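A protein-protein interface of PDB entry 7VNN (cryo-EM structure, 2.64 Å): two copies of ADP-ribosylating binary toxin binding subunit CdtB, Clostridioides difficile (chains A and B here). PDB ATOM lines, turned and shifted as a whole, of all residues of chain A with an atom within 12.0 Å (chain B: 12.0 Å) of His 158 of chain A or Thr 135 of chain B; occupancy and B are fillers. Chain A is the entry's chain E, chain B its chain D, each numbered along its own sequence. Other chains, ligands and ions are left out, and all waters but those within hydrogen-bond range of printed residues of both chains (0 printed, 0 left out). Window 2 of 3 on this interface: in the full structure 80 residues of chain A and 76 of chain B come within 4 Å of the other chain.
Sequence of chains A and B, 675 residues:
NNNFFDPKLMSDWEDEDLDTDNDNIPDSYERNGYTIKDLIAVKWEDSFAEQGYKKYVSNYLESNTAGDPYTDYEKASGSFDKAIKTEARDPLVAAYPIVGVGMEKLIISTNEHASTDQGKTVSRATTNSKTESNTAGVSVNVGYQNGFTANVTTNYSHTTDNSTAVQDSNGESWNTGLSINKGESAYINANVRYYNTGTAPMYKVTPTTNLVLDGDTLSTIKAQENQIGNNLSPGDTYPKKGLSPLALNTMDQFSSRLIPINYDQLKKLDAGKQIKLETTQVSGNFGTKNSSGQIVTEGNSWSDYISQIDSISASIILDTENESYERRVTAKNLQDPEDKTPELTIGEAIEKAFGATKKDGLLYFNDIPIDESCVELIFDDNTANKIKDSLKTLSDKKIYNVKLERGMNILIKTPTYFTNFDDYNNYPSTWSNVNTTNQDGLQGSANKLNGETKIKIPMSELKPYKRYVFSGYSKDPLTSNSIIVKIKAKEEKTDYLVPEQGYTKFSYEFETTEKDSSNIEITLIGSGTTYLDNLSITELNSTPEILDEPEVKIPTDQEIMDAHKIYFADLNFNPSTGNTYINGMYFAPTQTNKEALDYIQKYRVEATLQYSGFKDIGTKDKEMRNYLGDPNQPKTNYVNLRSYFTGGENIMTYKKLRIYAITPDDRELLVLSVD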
ATOM      1  N   LYS A 130       2.350  19.398  18.577  1.00  0.00           N
ATOM      2  CA  LYS A 130       3.408  18.942  19.465  1.00  0.00           C
ATOM      3  C   LYS A 130       3.873  17.566  19.012  1.00  0.00           C
ATOM      4  O   LYS A 130       3.054  16.719  18.644  1.00  0.00           O
ATOM      5  CB  LYS A 130       2.931  18.886  20.922  1.00  0.00           C
ATOM      6  CG  LYS A 130       2.719  20.248  21.560  1.00  0.00           C
ATOM      7  CD  LYS A 130       2.120  20.115  22.952  1.00  0.00           C
ATOM      8  CE  LYS A 130       3.098  19.455  23.912  1.00  0.00           C
ATOM      9  NZ  LYS A 130       2.550  19.373  25.294  1.00  0.00           N
ATOM     10  N   THR A 131       5.184  17.347  19.041  1.00  0.00           N
ATOM     11  CA  THR A 131       5.767  16.083  18.613  1.00  0.00           C
ATOM     12  C   THR A 131       6.907  15.703  19.544  1.00  0.00           C
ATOM     13  O   THR A 131       7.741  16.543  19.894  1.00  0.00           O
ATOM     14  CB  THR A 131       6.278  16.162  17.166  1.00  0.00           C
ATOM     15  OG1 THR A 131       5.265  16.737  16.330  1.00  0.00           O
ATOM     16  CG2 THR A 131       6.635  14.777  16.645  1.00  0.00           C
ATOM     17  N   GLU A 132       6.937  14.433  19.941  1.00  0.00           N
ATOM     18  CA  GLU A 132       7.965  13.895  20.829  1.00  0.00           C
ATOM     19  C   GLU A 132       8.645  12.735  20.109  1.00  0.00           C
ATOM     20  O   GLU A 132       8.186  11.592  20.184  1.00  0.00           O
ATOM     21  CB  GLU A 132       7.365  13.450  22.159  1.00  0.00           C
ATOM     22  CG  GLU A 132       6.297  14.384  22.703  1.00  0.00           C
ATOM     23  CD  GLU A 132       6.808  15.797  22.901  1.00  0.00           C
ATOM     24  OE1 GLU A 132       7.958  15.952  23.363  1.00  0.00           O
ATOM     25  OE2 GLU A 132       6.064  16.751  22.591  1.00  0.00           O
ATOM     26  N   SER A 133       9.744  13.028  19.419  1.00  0.00           N
ATOM     27  CA  SER A 133      10.448  12.026  18.633  1.00  0.00           C
ATOM     28  C   SER A 133      11.473  11.304  19.498  1.00  0.00           C
ATOM     29  O   SER A 133      12.287  11.942  20.175  1.00  0.00           O
ATOM     30  CB  SER A 133      11.127  12.669  17.423  1.00  0.00           C
ATOM     31  OG  SER A 133      11.829  11.702  16.662  1.00  0.00           O
ATOM     32  N   ASN A 134      11.426   9.975  19.474  1.00  0.00           N
ATOM     33  CA  ASN A 134      12.357   9.131  20.208  1.00  0.00           C
ATOM     34  C   ASN A 134      13.127   8.275  19.215  1.00  0.00           C
ATOM     35  O   ASN A 134      12.531   7.681  18.310  1.00  0.00           O
ATOM     36  CB  ASN A 134      11.625   8.244  21.219  1.00  0.00           C
ATOM     37  CG  ASN A 134      11.146   9.016  22.430  1.00  0.00           C
ATOM     38  OD1 ASN A 134      10.091   9.649  22.399  1.00  0.00           O
ATOM     39  ND2 ASN A 134      11.917   8.964  23.509  1.00  0.00           N
ATOM     40  N   THR A 135      14.443   8.217  19.382  1.00  0.00           N
ATOM     41  CA  THR A 135      15.291   7.434  18.493  1.00  0.00           C
ATOM     42  C   THR A 135      16.420   6.766  19.269  1.00  0.00           C
ATOM     43  O   THR A 135      16.195   6.175  20.325  1.00  0.00           O
ATOM     44  CB  THR A 135      15.884   8.304  17.368  1.00  0.00           C
ATOM     45  OG1 THR A 135      16.599   7.476  16.444  1.00  0.00           O
ATOM     46  CG2 THR A 135      16.822   9.353  17.942  1.00  0.00           C
ATOM     47  N   HIS A 158      16.408  12.056  20.935  1.00  0.00           N
ATOM     48  CA  HIS A 158      15.347  12.691  21.709  1.00  0.00           C
ATOM     49  C   HIS A 158      15.016  14.068  21.143  1.00  0.00           C
ATOM     50  O   HIS A 158      15.595  15.074  21.551  1.00  0.00           O
ATOM     51  CB  HIS A 158      15.750  12.803  23.181  1.00  0.00           C
ATOM     52  CG  HIS A 158      14.738  13.502  24.035  1.00  0.00           C
ATOM     53  ND1 HIS A 158      13.620  12.868  24.532  1.00  0.00           N
ATOM     54  CD2 HIS A 158      14.679  14.778  24.483  1.00  0.00           C
ATOM     55  CE1 HIS A 158      12.913  13.725  25.248  1.00  0.00           C
ATOM     56  NE2 HIS A 158      13.534  14.891  25.234  1.00  0.00           N
ATOM     57  N   THR A 159      14.083  14.106  20.197  1.00  0.00           N
ATOM     58  CA  THR A 159      13.681  15.338  19.536  1.00  0.00           C
ATOM     59  C   THR A 159      12.294  15.751  20.013  1.00  0.00           C
ATOM     60  O   THR A 159      11.398  14.911  20.148  1.00  0.00           O
ATOM     61  CB  THR A 159      13.682  15.173  18.013  1.00  0.00           C
ATOM     62  OG1 THR A 159      14.931  14.614  17.592  1.00  0.00           O
ATOM     63  CG2 THR A 159      13.490  16.518  17.332  1.00  0.00           C
ATOM     64  N   THR A 160      12.129  17.044  20.276  1.00  0.00           N
ATOM     65  CA  THR A 160      10.858  17.606  20.714  1.00  0.00           C
ATOM     66  C   THR A 160      10.663  18.948  20.026  1.00  0.00           C
ATOM     67  O   THR A 160      11.592  19.757  19.974  1.00  0.00           O
ATOM     68  CB  THR A 160      10.826  17.772  22.240  1.00  0.00           C
ATOM     69  OG1 THR A 160      10.713  16.484  22.858  1.00  0.00           O
ATOM     70  CG2 THR A 160       9.650  18.640  22.669  1.00  0.00           C
ATOM     71  N   ASP A 161       9.462  19.181  19.498  1.00  0.00           N
ATOM     72  CA  ASP A 161       9.177  20.399  18.752  1.00  0.00           C
ATOM     73  C   ASP A 161       7.797  20.926  19.119  1.00  0.00           C
ATOM     74  O   ASP A 161       7.032  20.287  19.846  1.00  0.00           O
ATOM     75  CB  ASP A 161       9.275  20.164  17.240  1.00  0.00           C
ATOM     76  CG  ASP A 161       8.452  18.985  16.780  1.00  0.00           C
ATOM     77  OD1 ASP A 161       8.984  17.856  16.788  1.00  0.00           O
ATOM     78  OD2 ASP A 161       7.278  19.185  16.404  1.00  0.00           O
ATOM     79  N   ASN A 162       7.492  22.119  18.607  1.00  0.00           N
ATOM     80  CA  ASN A 162       6.194  22.770  18.804  1.00  0.00           C
ATOM     81  C   ASN A 162       5.841  23.498  17.509  1.00  0.00           C
ATOM     82  O   ASN A 162       6.352  24.590  17.248  1.00  0.00           O
ATOM     83  CB  ASN A 162       6.224  23.734  19.986  1.00  0.00           C
ATOM     84  CG  ASN A 162       6.116  23.026  21.321  1.00  0.00           C
ATOM     85  OD1 ASN A 162       7.052  22.360  21.764  1.00  0.00           O
ATOM     86  ND2 ASN A 162       4.969  23.171  21.974  1.00  0.00           N
ATOM     87  N   THR B 131       7.892  27.062  13.934  1.00  0.00           N
ATOM     88  CA  THR B 131       8.156  25.880  14.741  1.00  0.00           C
ATOM     89  C   THR B 131       9.395  26.106  15.597  1.00  0.00           C
ATOM     90  O   THR B 131      10.317  26.826  15.207  1.00  0.00           O
ATOM     91  CB  THR B 131       8.349  24.634  13.862  1.00  0.00           C
ATOM     92  OG1 THR B 131       7.337  24.601  12.848  1.00  0.00           O
ATOM     93  CG2 THR B 131       8.256  23.364  14.695  1.00  0.00           C
ATOM     94  N   GLU B 132       9.402  25.479  16.775  1.00  0.00           N
ATOM     95  CA  GLU B 132      10.545  25.497  17.684  1.00  0.00           C
ATOM     96  C   GLU B 132      10.883  24.057  18.048  1.00  0.00           C
ATOM     97  O   GLU B 132      10.182  23.439  18.854  1.00  0.00           O
ATOM     98  CB  GLU B 132      10.245  26.318  18.938  1.00  0.00           C
ATOM     99  CG  GLU B 132      10.053  27.800  18.680  1.00  0.00           C
ATOM    100  CD  GLU B 132      11.349  28.496  18.313  1.00  0.00           C
ATOM    101  OE1 GLU B 132      12.393  28.164  18.911  1.00  0.00           O
ATOM    102  OE2 GLU B 132      11.322  29.373  17.424  1.00  0.00           O
ATOM    103  N   SER B 133      11.955  23.531  17.464  1.00  0.00           N
ATOM    104  CA  SER B 133      12.364  22.147  17.656  1.00  0.00           C
ATOM    105  C   SER B 133      13.698  22.100  18.388  1.00  0.00           C
ATOM    106  O   SER B 133      14.621  22.852  18.064  1.00  0.00           O
ATOM    107  CB  SER B 133      12.475  21.417  16.312  1.00  0.00           C
ATOM    108  OG  SER B 133      12.750  20.040  16.499  1.00  0.00           O
ATOM    109  N   ASN B 134      13.794  21.211  19.378  1.00  0.00           N
ATOM    110  CA  ASN B 134      14.998  21.055  20.180  1.00  0.00           C
ATOM    111  C   ASN B 134      15.378  19.584  20.260  1.00  0.00           C
ATOM    112  O   ASN B 134      14.516  18.701  20.236  1.00  0.00           O
ATOM    113  CB  ASN B 134      14.813  21.611  21.600  1.00  0.00           C
ATOM    114  CG  ASN B 134      14.754  23.124  21.630  1.00  0.00           C
ATOM    115  OD1 ASN B 134      15.784  23.797  21.669  1.00  0.00           O
ATOM    116  ND2 ASN B 134      13.542  23.669  21.617  1.00  0.00           N
ATOM    117  N   THR B 135      16.681  19.331  20.361  1.00  0.00           N
ATOM    118  CA  THR B 135      17.197  17.969  20.465  1.00  0.00           C
ATOM    119  C   THR B 135      18.616  17.950  21.028  1.00  0.00           C
ATOM    120  O   THR B 135      19.348  18.936  20.931  1.00  0.00           O
ATOM    121  CB  THR B 135      17.192  17.258  19.101  1.00  0.00           C
ATOM    122  OG1 THR B 135      17.771  15.953  19.238  1.00  0.00           O
ATOM    123  CG2 THR B 135      17.987  18.058  18.081  1.00  0.00           C
ATOM    124  N   HIS B 158      18.466  22.728  18.359  1.00  0.00           N
ATOM    125  CA  HIS B 158      17.594  23.876  18.570  1.00  0.00           C
ATOM    126  C   HIS B 158      17.343  24.582  17.243  1.00  0.00           C
ATOM    127  O   HIS B 158      17.968  25.597  16.938  1.00  0.00           O
ATOM    128  CB  HIS B 158      18.212  24.836  19.591  1.00  0.00           C
ATOM    129  CG  HIS B 158      17.358  26.027  19.899  1.00  0.00           C
ATOM    130  ND1 HIS B 158      16.342  25.991  20.830  1.00  0.00           N
ATOM    131  CD2 HIS B 158      17.378  27.290  19.411  1.00  0.00           C
ATOM    132  CE1 HIS B 158      15.767  27.178  20.896  1.00  0.00           C
ATOM    133  NE2 HIS B 158      16.377  27.984  20.045  1.00  0.00           N
ATOM    134  N   THR B 159      16.421  24.035  16.456  1.00  0.00           N
ATOM    135  CA  THR B 159      16.144  24.507  15.108  1.00  0.00           C
ATOM    136  C   THR B 159      14.860  25.323  15.088  1.00  0.00           C
ATOM    137  O   THR B 159      13.849  24.925  15.676  1.00  0.00           O
ATOM    138  CB  THR B 159      16.023  23.336  14.126  1.00  0.00           C
ATOM    139  OG1 THR B 159      17.132  22.446  14.302  1.00  0.00           O
ATOM    140  CG2 THR B 159      16.010  23.841  12.689  1.00  0.00           C
ATOM    141  N   THR B 160      14.910  26.468  14.409  1.00  0.00           N
ATOM    142  CA  THR B 160      13.755  27.337  14.226  1.00  0.00           C
ATOM    143  C   THR B 160      13.526  27.538  12.736  1.00  0.00           C
ATOM    144  O   THR B 160      14.426  27.996  12.024  1.00  0.00           O
ATOM    145  CB  THR B 160      13.961  28.689  14.920  1.00  0.00           C
ATOM    146  OG1 THR B 160      13.801  28.535  16.335  1.00  0.00           O
ATOM    147  CG2 THR B 160      12.957  29.712  14.410  1.00  0.00           C
ATOM    148  N   ASP B 161      12.327  27.197  12.267  1.00  0.00           N
ATOM    149  CA  ASP B 161      11.977  27.330  10.861  1.00  0.00           C
ATOM    150  C   ASP B 161      10.709  28.160  10.720  1.00  0.00           C
ATOM    151  O   ASP B 161       9.766  28.026  11.504  1.00  0.00           O
ATOM    152  CB  ASP B 161      11.795  25.954  10.192  1.00  0.00           C
ATOM    153  CG  ASP B 161      10.653  25.154  10.792  1.00  0.00           C
ATOM    154  OD1 ASP B 161       9.484  25.418  10.437  1.00  0.00           O
ATOM    155  OD2 ASP B 161      10.925  24.256  11.618  1.00  0.00           O
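N of Asn 162 of chain A sits at hydrogen-bond distance from O of Glu 132 of chain B, at 3.0 Å. OG1 of Thr 135 of chain B is in hydrogen-bond range of O of His 158 of chain A (3.3 Å). The backbone NH (N) of Asn 134 of chain B lies within hydrogen-bond range of the backbone carbonyl oxygen (O) of Thr 160 of chain A (2.7 Å).
Along chain A the printed residues that touch a printed residue of chain B span positions 158 to 162. Among the printed residues, no Asp or Glu carboxylate lies within 4 Å of a Lys or Arg side-chain nitrogen of the other chain.
Ser 133 of chain B touches Thr 159 of chain A (OG to CG2, 3.7 Å). Thr 159 of chain A touches Asn 134 of chain B. Thr 159 of chain A touches Thr 135 of chain B (OG1 to OG1, 3.5 Å). Thr 160 of chain A touches Ser 133 of chain B. CA of Asp 161 of chain A touches O of Glu 132 of chain B (3.2 Å). Ser 133 of chain B touches Asp 161 of chain A. Thr 131 of chain B touches Asn 162 of chain A (CA to O, 3.3 Å).
His 158 of chain A touches Thr 135 of chain B, but with the chains exchanged Thr 135 of chain A does not touch His 158 of chain B (13.5 Å). Thr 159 of chain A touches Asn 134 of chain B, but with the chains exchanged Asn 134 of chain A does not touch Thr 159 of chain B (14.7 Å). Thr 160 of chain A touches Asn 134 of chain B, but with the chains exchanged Asn 134 of chain A does not touch Thr 160 of chain B (17.6 Å). Asp 161 of chain A touches Glu 132 of chain B, but with the chains exchanged Glu 132 of chain A does not touch Asp 161 of chain B (13.5 Å). Positions printed for both chains: 131, 132, 133, 134, 135, 158, 159, 160 and 161.
Of the printed residues of chain B, His 158 of chain A touches Thr 135 (3.3 Å). Of chain A, only His 158 (3.3 Å) and Thr 159 (3.5 Å) come within 4 Å of Thr 135 of chain B. No residue of chain B comes within 4 Å of Ser 133 of chain A. No residue of chain B comes within 4 Å of Asn 134 of chain A. No residue of chain B comes within 4 Å of Thr 135 of chain A. Thr 160 of chain A touches two residues of chain B. Of the printed residues of chain A, Asn 134 of chain B touches Thr 159 (3.5 Å) and Thr 160 (2.7 Å). Of the printed residues of chain B, Asn 162 of chain A touches Thr 131 (3.3 Å) and Glu 132 (3.0 Å). Printed residues of chain A within 4 Å of Thr 131 of chain B: Asn 162. Printed residues of chain B within 4 Å of Asp 161 of chain A: Glu 132 and Ser 133. Of the printed residues of chain A, Glu 132 of chain B touches Asp 161 and Asn 162. The nearest printed residue of chain B that does not touch His 158 of chain A is Asn 134 of chain B (4.01 Å).
O of Ser 133 of chain B sits at hydrogen-bond distance from N of Thr 159 of chain B, 2.7 Å away. OE1 of Glu 132 of chain A sits at hydrogen-bond distance from OG1 of Thr 160 of chain A (2.9 Å). A ring nitrogen (ND1) of His 158 of chain B lies within hydrogen-bond range of the side-chain amide oxygen of Asn 134 of chain B (2.4 Å). OG1 of Thr 160 of chain B is in hydrogen-bond range of OE2 of Glu 132 of chain B. OD2 of Asp 161 of chain A sits at hydrogen-bond distance from OG1 of Thr 131 of chain A. The backbone NH (N) of Ser 133 of chain A is in hydrogen-bond range of the backbone carbonyl oxygen (O) of Thr 159 of chain A (2.6 Å).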
